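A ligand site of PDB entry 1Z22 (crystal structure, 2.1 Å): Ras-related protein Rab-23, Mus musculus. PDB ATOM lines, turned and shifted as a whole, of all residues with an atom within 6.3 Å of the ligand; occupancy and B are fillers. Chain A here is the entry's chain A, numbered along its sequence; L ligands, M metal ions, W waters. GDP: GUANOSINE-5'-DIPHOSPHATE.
Water W2 lies within hydrogen-bond range of O2' of the ligand (2.6 Å) and O of Lys 32 (3.2 Å). Water W4 lies within hydrogen-bond range of O of Thr 31 (2.5 Å), O2' of the ligand (2.7 Å) and OG of Ser 20 (2.7 Å). Water W6 lies within hydrogen-bond range of the side-chain amino group (NZ) of Lys 18 and an oxygen (O1B) of the ligand. Water W9 bridges OG of Ser 19 (3.0 Å) and O3B of the ligand (3.1 Å). Water W3 bridges the side-chain amino group of Lys 118 (3.1 Å) and a nitrogen (N3) of the ligand (3.3 Å).
The side-chain amino group of Lys 18 lies close to the backbone carbonyl oxygen of Gly 12, 3.4 Å away. NZ of Lys 18 lies within hydrogen-bond range of O of Asn 13 (2.8 Å). The side-chain amino group (NZ) of Lys 118 lies within hydrogen-bond range of the backbone carbonyl oxygen (O) of Ala 15 (2.7 Å). The backbone carbonyl oxygen (O) of Thr 146 is in hydrogen-bond range of the side-chain amide nitrogen (ND2) of Asn 117, 3.2 Å away. The backbone NH of Val 148 lies close to the side-chain amide nitrogen of Asn 117, at 3.2 Å. The side-chain hydroxyl of Ser 147 lies within hydrogen-bond range of the backbone NH of Glu 150, 3.1 Å away. O of Thr 146 lies within hydrogen-bond range of N of Lys 118. OD1 of Asp 120 sits at hydrogen-bond distance from OG of Ser 147, 2.7 Å away.
Gly 14 touches the ligand (C to O1B, 3.8 Å). Phe 30 touches the ligand (CZ to O2', 3.4 Å). Thr 31 touches the ligand. CD1 of Leu 121 touches N2 of the ligand, 3.6 Å away. C of Ser 147 touches O6 of the ligand, at 3.6 Å. Hydrophobic or aromatic side chains that line the ligand: Val 16, Phe 30, Leu 121 and Val 148. Within 4 Å of the ligand: Gly 14, Ala 15, Val 16, Gly 17, Lys 18, Ser 19, Ser 20, Phe 30, Thr 31, Asn 117, Lys 118, Asp 120, Leu 121, Ser 147, Val 148 and Lys 149.
O2B of the ligand sits at hydrogen-bond distance from N of Lys 18 (2.8 Å). O6 of the ligand lies within hydrogen-bond range of N of Val 148 (2.9 Å). The side-chain amino group (NZ) of Lys 118 is in hydrogen-bond range of an oxygen (O4') of the ligand (3.1 Å). OD1 of Asp 120 sits at hydrogen-bond distance from N1 of the ligand (2.8 Å). The backbone NH (N) of Ser 20 sits at hydrogen-bond distance from an oxygen (O2A) of the ligand. An oxygen (O2B) of the ligand lies within salt-bridge range of the side-chain amino group (NZ) of Lys 18, at 2.5 Å. An oxygen (O3A) of the ligand lies within hydrogen-bond range of the backbone NH (N) of Gly 17 (3.1 Å). An oxygen (O2B) of the ligand sits at hydrogen-bond distance from the backbone NH of Val 16 (3.4 Å). N of Ser 19 lies within hydrogen-bond range of O3B of the ligand (3.0 Å). The side-chain hydroxyl of Ser 20 is in hydrogen-bond range of an oxygen (O2A) of the ligand. The side-chain hydroxyl (OG) of Ser 19 lies within hydrogen-bond range of an oxygen (O3B) of the ligand (2.8 Å). OD1 of Asn 117 sits close to N7 of the ligand. The backbone NH (N) of Lys 149 lies within hydrogen-bond range of an oxygen (O6) of the ligand (3.1 Å). O1B of the ligand lies within hydrogen-bond range of N of Ala 15 (2.8 Å).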
ATOM      1  N   GLY A  12      26.660 -17.623  13.780  1.00  0.00           N
ATOM      2  CA  GLY A  12      26.443 -17.673  15.218  1.00  0.00           C
ATOM      3  C   GLY A  12      27.019 -18.906  15.879  1.00  0.00           C
ATOM      4  O   GLY A  12      27.498 -19.811  15.206  1.00  0.00           O
ATOM      5  N   ASN A  13      26.959 -18.939  17.214  1.00  0.00           N
ATOM      6  CA  ASN A  13      27.454 -20.076  18.000  1.00  0.00           C
ATOM      7  C   ASN A  13      26.695 -21.359  17.673  1.00  0.00           C
ATOM      8  O   ASN A  13      25.610 -21.319  17.095  1.00  0.00           O
ATOM      9  CB  ASN A  13      27.351 -19.786  19.501  1.00  0.00           C
ATOM     10  CG  ASN A  13      28.526 -18.969  20.035  1.00  0.00           C
ATOM     11  OD1 ASN A  13      29.255 -18.314  19.287  1.00  0.00           O
ATOM     12  ND2 ASN A  13      28.714 -19.002  21.353  1.00  0.00           N
ATOM     13  N   GLY A  14      27.270 -22.495  18.044  1.00  0.00           N
ATOM     14  CA  GLY A  14      26.616 -23.784  17.834  1.00  0.00           C
ATOM     15  C   GLY A  14      25.285 -23.852  18.544  1.00  0.00           C
ATOM     16  O   GLY A  14      25.108 -23.260  19.606  1.00  0.00           O
ATOM     17  N   ALA A  15      24.322 -24.546  17.922  1.00  0.00           N
ATOM     18  CA  ALA A  15      23.035 -24.888  18.533  1.00  0.00           C
ATOM     19  C   ALA A  15      22.048 -23.722  18.731  1.00  0.00           C
ATOM     20  O   ALA A  15      21.030 -23.891  19.410  1.00  0.00           O
ATOM     21  CB  ALA A  15      23.238 -25.678  19.854  1.00  0.00           C
ATOM     22  N   VAL A  16      22.324 -22.582  18.105  1.00  0.00           N
ATOM     23  CA  VAL A  16      21.422 -21.422  18.183  1.00  0.00           C
ATOM     24  C   VAL A  16      20.182 -21.581  17.289  1.00  0.00           C
ATOM     25  O   VAL A  16      19.179 -20.885  17.490  1.00  0.00           O
ATOM     26  CB  VAL A  16      22.152 -20.080  17.896  1.00  0.00           C
ATOM     27  CG1 VAL A  16      23.260 -19.851  18.925  1.00  0.00           C
ATOM     28  CG2 VAL A  16      22.701 -20.025  16.471  1.00  0.00           C
ATOM     29  N   GLY A  17      20.252 -22.489  16.331  1.00  0.00           N
ATOM     30  CA  GLY A  17      19.169 -22.750  15.394  1.00  0.00           C
ATOM     31  C   GLY A  17      19.459 -22.361  13.951  1.00  0.00           C
ATOM     32  O   GLY A  17      18.531 -22.172  13.180  1.00  0.00           O
ATOM     33  N   LYS A  18      20.732 -22.284  13.569  1.00  0.00           N
ATOM     34  CA  LYS A  18      21.123 -21.825  12.212  1.00  0.00           C
ATOM     35  C   LYS A  18      20.656 -22.727  11.071  1.00  0.00           C
ATOM     36  O   LYS A  18      20.011 -22.261  10.141  1.00  0.00           O
ATOM     37  CB  LYS A  18      22.640 -21.640  12.113  1.00  0.00           C
ATOM     38  CG  LYS A  18      23.223 -20.547  13.014  1.00  0.00           C
ATOM     39  CD  LYS A  18      24.746 -20.392  12.840  1.00  0.00           C
ATOM     40  CE  LYS A  18      25.527 -21.670  13.151  1.00  0.00           C
ATOM     41  NZ  LYS A  18      25.167 -22.217  14.493  1.00  0.00           N
ATOM     42  N   SER A  19      20.992 -24.017  11.132  1.00  0.00           N
ATOM     43  CA  SER A  19      20.599 -24.982  10.114  1.00  0.00           C
ATOM     44  C   SER A  19      19.083 -25.161  10.103  1.00  0.00           C
ATOM     45  O   SER A  19      18.464 -25.242   9.021  1.00  0.00           O
ATOM     46  CB  SER A  19      21.307 -26.332  10.305  1.00  0.00           C
ATOM     47  OG  SER A  19      21.077 -26.837  11.612  1.00  0.00           O
ATOM     48  N   SER A  20      18.486 -25.213  11.290  1.00  0.00           N
ATOM     49  CA  SER A  20      17.033 -25.229  11.421  1.00  0.00           C
ATOM     50  C   SER A  20      16.372 -24.017  10.760  1.00  0.00           C
ATOM     51  O   SER A  20      15.329 -24.156  10.110  1.00  0.00           O
ATOM     52  CB  SER A  20      16.602 -25.317  12.893  1.00  0.00           C
ATOM     53  OG  SER A  20      16.929 -26.577  13.450  1.00  0.00           O
ATOM     54  N   MET A  21      16.971 -22.836  10.920  1.00  0.00           N
ATOM     55  CA  MET A  21      16.416 -21.615  10.311  1.00  0.00           C
ATOM     56  C   MET A  21      16.369 -21.760   8.795  1.00  0.00           C
ATOM     57  O   MET A  21      15.369 -21.430   8.160  1.00  0.00           O
ATOM     58  CB  MET A  21      17.221 -20.378  10.714  1.00  0.00           C
ATOM     59  CG  MET A  21      16.513 -19.064  10.374  1.00  0.00           C
ATOM     60  SD  MET A  21      17.441 -17.601  10.906  1.00  0.00           S
ATOM     61  CE  MET A  21      16.229 -16.315  10.627  1.00  0.00           C
ATOM     62  N   PHE A  30      10.227 -28.191  10.215  1.00  0.00           N
ATOM     63  CA  PHE A  30      10.999 -28.180  11.449  1.00  0.00           C
ATOM     64  C   PHE A  30      11.085 -29.605  11.985  1.00  0.00           C
ATOM     65  O   PHE A  30      10.055 -30.260  12.205  1.00  0.00           O
ATOM     66  CB  PHE A  30      10.377 -27.253  12.497  1.00  0.00           C
ATOM     67  CG  PHE A  30      11.105 -27.254  13.812  1.00  0.00           C
ATOM     68  CD1 PHE A  30      12.304 -26.560  13.961  1.00  0.00           C
ATOM     69  CD2 PHE A  30      10.584 -27.945  14.913  1.00  0.00           C
ATOM     70  CE1 PHE A  30      12.983 -26.556  15.195  1.00  0.00           C
ATOM     71  CE2 PHE A  30      11.263 -27.951  16.136  1.00  0.00           C
ATOM     72  CZ  PHE A  30      12.455 -27.260  16.279  1.00  0.00           C
ATOM     73  N   THR A  31      12.314 -30.080  12.185  1.00  0.00           N
ATOM     74  CA  THR A  31      12.581 -31.428  12.685  1.00  0.00           C
ATOM     75  C   THR A  31      12.964 -31.365  14.164  1.00  0.00           C
ATOM     76  O   THR A  31      13.961 -30.739  14.528  1.00  0.00           O
ATOM     77  CB  THR A  31      13.737 -32.105  11.896  1.00  0.00           C
ATOM     78  OG1 THR A  31      13.496 -31.989  10.483  1.00  0.00           O
ATOM     79  CG2 THR A  31      13.857 -33.579  12.282  1.00  0.00           C
ATOM     80  N   LYS A  32      12.177 -32.041  14.999  1.00  0.00           N
ATOM     81  CA  LYS A  32      12.428 -32.079  16.433  1.00  0.00           C
ATOM     82  C   LYS A  32      13.646 -32.922  16.807  1.00  0.00           C
ATOM     83  O   LYS A  32      14.467 -32.504  17.636  1.00  0.00           O
ATOM     84  CB  LYS A  32      11.182 -32.579  17.169  1.00  0.00           C
ATOM     85  N   ASP A  33      13.780 -34.093  16.172  1.00  0.00           N
ATOM     86  CA  ASP A  33      14.756 -35.108  16.566  1.00  0.00           C
ATOM     87  C   ASP A  33      16.225 -34.778  16.256  1.00  0.00           C
ATOM     88  O   ASP A  33      17.121 -35.190  17.007  1.00  0.00           O
ATOM     89  CB  ASP A  33      14.372 -36.458  15.971  1.00  0.00           C
ATOM     90  N   TYR A  34      16.470 -34.078  15.147  1.00  0.00           N
ATOM     91  CA  TYR A  34      17.816 -33.654  14.719  1.00  0.00           C
ATOM     92  C   TYR A  34      18.722 -34.789  14.219  1.00  0.00           C
ATOM     93  O   TYR A  34      19.929 -34.583  14.009  1.00  0.00           O
ATOM     94  CB  TYR A  34      18.513 -32.832  15.816  1.00  0.00           C
ATOM     95  N   ASP A  60      25.118 -22.032   5.793  1.00  0.00           N
ATOM     96  CA  ASP A  60      25.281 -22.131   7.239  1.00  0.00           C
ATOM     97  C   ASP A  60      26.772 -22.142   7.548  1.00  0.00           C
ATOM     98  O   ASP A  60      27.451 -23.112   7.223  1.00  0.00           O
ATOM     99  CB  ASP A  60      24.602 -23.419   7.739  1.00  0.00           C
ATOM    100  CG  ASP A  60      24.856 -23.685   9.218  1.00  0.00           C
ATOM    101  OD1 ASP A  60      25.375 -22.797   9.920  1.00  0.00           O
ATOM    102  OD2 ASP A  60      24.533 -24.798   9.676  1.00  0.00           O
ATOM    103  N   ASN A 117      16.801 -16.214  18.268  1.00  0.00           N
ATOM    104  CA  ASN A 117      16.012 -17.393  17.945  1.00  0.00           C
ATOM    105  C   ASN A 117      15.532 -18.099  19.214  1.00  0.00           C
ATOM    106  O   ASN A 117      15.987 -17.769  20.319  1.00  0.00           O
ATOM    107  CB  ASN A 117      16.830 -18.351  17.055  1.00  0.00           C
ATOM    108  CG  ASN A 117      15.987 -19.499  16.500  1.00  0.00           C
ATOM    109  OD1 ASN A 117      16.458 -20.634  16.426  1.00  0.00           O
ATOM    110  ND2 ASN A 117      14.757 -19.211  16.113  1.00  0.00           N
ATOM    111  N   LYS A 118      14.611 -19.048  19.042  1.00  0.00           N
ATOM    112  CA  LYS A 118      13.995 -19.813  20.139  1.00  0.00           C
ATOM    113  C   LYS A 118      13.138 -18.938  21.065  1.00  0.00           C
ATOM    114  O   LYS A 118      12.982 -19.232  22.259  1.00  0.00           O
ATOM    115  CB  LYS A 118      15.036 -20.619  20.956  1.00  0.00           C
ATOM    116  CG  LYS A 118      16.046 -21.381  20.110  1.00  0.00           C
ATOM    117  CD  LYS A 118      16.836 -22.404  20.936  1.00  0.00           C
ATOM    118  CE  LYS A 118      17.944 -23.035  20.088  1.00  0.00           C
ATOM    119  NZ  LYS A 118      18.711 -24.104  20.816  1.00  0.00           N
ATOM    120  N   ILE A 119      12.554 -17.875  20.493  1.00  0.00           N
ATOM    121  CA  ILE A 119      11.715 -16.939  21.251  1.00  0.00           C
ATOM    122  C   ILE A 119      10.428 -17.592  21.793  1.00  0.00           C
ATOM    123  O   ILE A 119       9.762 -17.034  22.657  1.00  0.00           O
ATOM    124  CB  ILE A 119      11.406 -15.644  20.439  1.00  0.00           C
ATOM    125  CG1 ILE A 119      11.129 -14.461  21.369  1.00  0.00           C
ATOM    126  CG2 ILE A 119      10.276 -15.875  19.421  1.00  0.00           C
ATOM    127  CD1 ILE A 119      12.288 -14.090  22.275  1.00  0.00           C
ATOM    128  N   ASP A 120      10.107 -18.788  21.294  1.00  0.00           N
ATOM    129  CA  ASP A 120       9.032 -19.602  21.869  1.00  0.00           C
ATOM    130  C   ASP A 120       9.329 -20.006  23.316  1.00  0.00           C
ATOM    131  O   ASP A 120       8.425 -20.330  24.079  1.00  0.00           O
ATOM    132  CB  ASP A 120       8.745 -20.851  21.013  1.00  0.00           C
ATOM    133  CG  ASP A 120      10.005 -21.664  20.723  1.00  0.00           C
ATOM    134  OD1 ASP A 120      10.831 -21.223  19.894  1.00  0.00           O
ATOM    135  OD2 ASP A 120      10.163 -22.747  21.322  1.00  0.00           O
ATOM    136  N   LEU A 121      10.624 -19.966  23.680  1.00  0.00           N
ATOM    137  CA  LEU A 121      11.090 -20.278  25.028  1.00  0.00           C
ATOM    138  C   LEU A 121      11.355 -19.024  25.873  1.00  0.00           C
ATOM    139  O   LEU A 121      12.068 -19.087  26.883  1.00  0.00           O
ATOM    140  CB  LEU A 121      12.359 -21.143  24.971  1.00  0.00           C
ATOM    141  CG  LEU A 121      12.364 -22.386  24.076  1.00  0.00           C
ATOM    142  CD1 LEU A 121      13.758 -23.004  24.043  1.00  0.00           C
ATOM    143  CD2 LEU A 121      11.329 -23.404  24.545  1.00  0.00           C
ATOM    144  N   THR A 146      12.717 -14.395  16.976  1.00  0.00           N
ATOM    145  CA  THR A 146      12.329 -15.429  16.017  1.00  0.00           C
ATOM    146  C   THR A 146      12.070 -16.790  16.682  1.00  0.00           C
ATOM    147  O   THR A 146      12.747 -17.160  17.628  1.00  0.00           O
ATOM    148  CB  THR A 146      13.447 -15.582  14.958  1.00  0.00           C
ATOM    149  OG1 THR A 146      13.550 -14.375  14.191  1.00  0.00           O
ATOM    150  CG2 THR A 146      13.179 -16.736  13.996  1.00  0.00           C
ATOM    151  N   SER A 147      11.063 -17.505  16.182  1.00  0.00           N
ATOM    152  CA  SER A 147      10.896 -18.913  16.519  1.00  0.00           C
ATOM    153  C   SER A 147      10.864 -19.761  15.247  1.00  0.00           C
ATOM    154  O   SER A 147       9.863 -19.768  14.526  1.00  0.00           O
ATOM    155  CB  SER A 147       9.654 -19.163  17.360  1.00  0.00           C
ATOM    156  OG  SER A 147       9.545 -20.550  17.662  1.00  0.00           O
ATOM    157  N   VAL A 148      11.975 -20.427  14.959  1.00  0.00           N
ATOM    158  CA  VAL A 148      12.036 -21.382  13.869  1.00  0.00           C
ATOM    159  C   VAL A 148      11.034 -22.516  14.098  1.00  0.00           C
ATOM    160  O   VAL A 148      10.333 -22.938  13.173  1.00  0.00           O
ATOM    161  CB  VAL A 148      13.469 -21.951  13.685  1.00  0.00           C
ATOM    162  CG1 VAL A 148      13.461 -23.161  12.749  1.00  0.00           C
ATOM    163  CG2 VAL A 148      14.393 -20.880  13.162  1.00  0.00           C
ATOM    164  N   LYS A 149      10.955 -22.976  15.342  1.00  0.00           N
ATOM    165  CA  LYS A 149      10.005 -24.007  15.749  1.00  0.00           C
ATOM    166  C   LYS A 149       8.558 -23.664  15.388  1.00  0.00           C
ATOM    167  O   LYS A 149       7.799 -24.513  14.909  1.00  0.00           O
ATOM    168  CB  LYS A 149      10.111 -24.271  17.256  1.00  0.00           C
ATOM    169  CG  LYS A 149       9.165 -25.354  17.762  1.00  0.00           C
ATOM    170  CD  LYS A 149       9.383 -25.631  19.241  1.00  0.00           C
ATOM    171  CE  LYS A 149       8.183 -26.398  19.803  1.00  0.00           C
ATOM    172  NZ  LYS A 149       8.403 -26.804  21.209  1.00  0.00           N
ATOM    173  N   GLU A 150       8.169 -22.412  15.628  1.00  0.00           N
ATOM    174  CA  GLU A 150       6.780 -22.011  15.434  1.00  0.00           C
ATOM    175  C   GLU A 150       6.587 -21.150  14.193  1.00  0.00           C
ATOM    176  O   GLU A 150       5.494 -20.654  13.947  1.00  0.00           O
ATOM    177  CB  GLU A 150       6.231 -21.312  16.683  1.00  0.00           C
ATOM    178  CG  GLU A 150       6.297 -22.167  17.958  1.00  0.00           C
ATOM    179  CD  GLU A 150       5.473 -23.446  17.885  1.00  0.00           C
ATOM    180  OE1 GLU A 150       4.519 -23.510  17.090  1.00  0.00           O
ATOM    181  OE2 GLU A 150       5.778 -24.386  18.638  1.00  0.00           O
HETATM  182  PB  GDP L   1      22.796 -24.901  14.785  1.00  0.00           P
HETATM  183  O1B GDP L   1      23.993 -25.575  15.387  1.00  0.00           O
HETATM  184  O2B GDP L   1      22.964 -23.410  14.896  1.00  0.00           O
HETATM  185  O3B GDP L   1      22.645 -25.305  13.330  1.00  0.00           O
HETATM  186  O3A GDP L   1      21.484 -25.298  15.622  1.00  0.00           O
HETATM  187  PA  GDP L   1      20.350 -26.318  15.104  1.00  0.00           P
HETATM  188  O1A GDP L   1      20.940 -27.667  14.797  1.00  0.00           O
HETATM  189  O2A GDP L   1      19.613 -25.736  13.934  1.00  0.00           O
HETATM  190  O5' GDP L   1      19.375 -26.404  16.388  1.00  0.00           O
HETATM  191  C5' GDP L   1      19.864 -26.824  17.657  1.00  0.00           C
HETATM  192  C4' GDP L   1      18.703 -27.318  18.509  1.00  0.00           C
HETATM  193  O4' GDP L   1      17.818 -26.217  18.795  1.00  0.00           O
HETATM  194  C3' GDP L   1      17.880 -28.372  17.779  1.00  0.00           C
HETATM  195  O3' GDP L   1      17.398 -29.326  18.730  1.00  0.00           O
HETATM  196  C2' GDP L   1      16.717 -27.576  17.227  1.00  0.00           C
HETATM  197  O2' GDP L   1      15.548 -28.392  17.033  1.00  0.00           O
HETATM  198  C1' GDP L   1      16.505 -26.516  18.297  1.00  0.00           C
HETATM  199  N9  GDP L   1      15.842 -25.310  17.763  1.00  0.00           N
HETATM  200  C8  GDP L   1      16.129 -24.629  16.631  1.00  0.00           C
HETATM  201  N7  GDP L   1      15.295 -23.567  16.480  1.00  0.00           N
HETATM  202  C5  GDP L   1      14.445 -23.577  17.538  1.00  0.00           C
HETATM  203  C6  GDP L   1      13.320 -22.747  18.013  1.00  0.00           C
HETATM  204  O6  GDP L   1      12.931 -21.752  17.363  1.00  0.00           O
HETATM  205  N1  GDP L   1      12.730 -23.099  19.165  1.00  0.00           N
HETATM  206  C2  GDP L   1      13.121 -24.171  19.898  1.00  0.00           C
HETATM  207  N2  GDP L   1      12.450 -24.437  21.043  1.00  0.00           N
HETATM  208  N3  GDP L   1      14.141 -24.973  19.520  1.00  0.00           N
HETATM  209  C4  GDP L   1      14.825 -24.724  18.370  1.00  0.00           C
HETATM  210 MG    MG M   1      25.075 -25.598  12.021  1.00  0.00          MG
HETATM  211  O   HOH W   1      19.385 -29.772  14.649  1.00  0.00           O
HETATM  212  O   HOH W   2      14.116 -29.538  18.872  1.00  0.00           O
HETATM  213  O   HOH W   3      16.372 -25.857  21.801  1.00  0.00           O
HETATM  214  O   HOH W   4      15.568 -28.781  14.361  1.00  0.00           O
HETATM  215  O   HOH W   5      24.050 -28.122  16.624  1.00  0.00           O
HETATM  216  O   HOH W   6      26.683 -24.661  14.351  1.00  0.00           O
HETATM  217  O   HOH W   7      22.372 -29.102  18.418  1.00  0.00           O
HETATM  218  O   HOH W   8      12.228 -26.726  22.493  1.00  0.00           O
HETATM  219  O   HOH W   9      23.388 -28.266  12.887  1.00  0.00           O
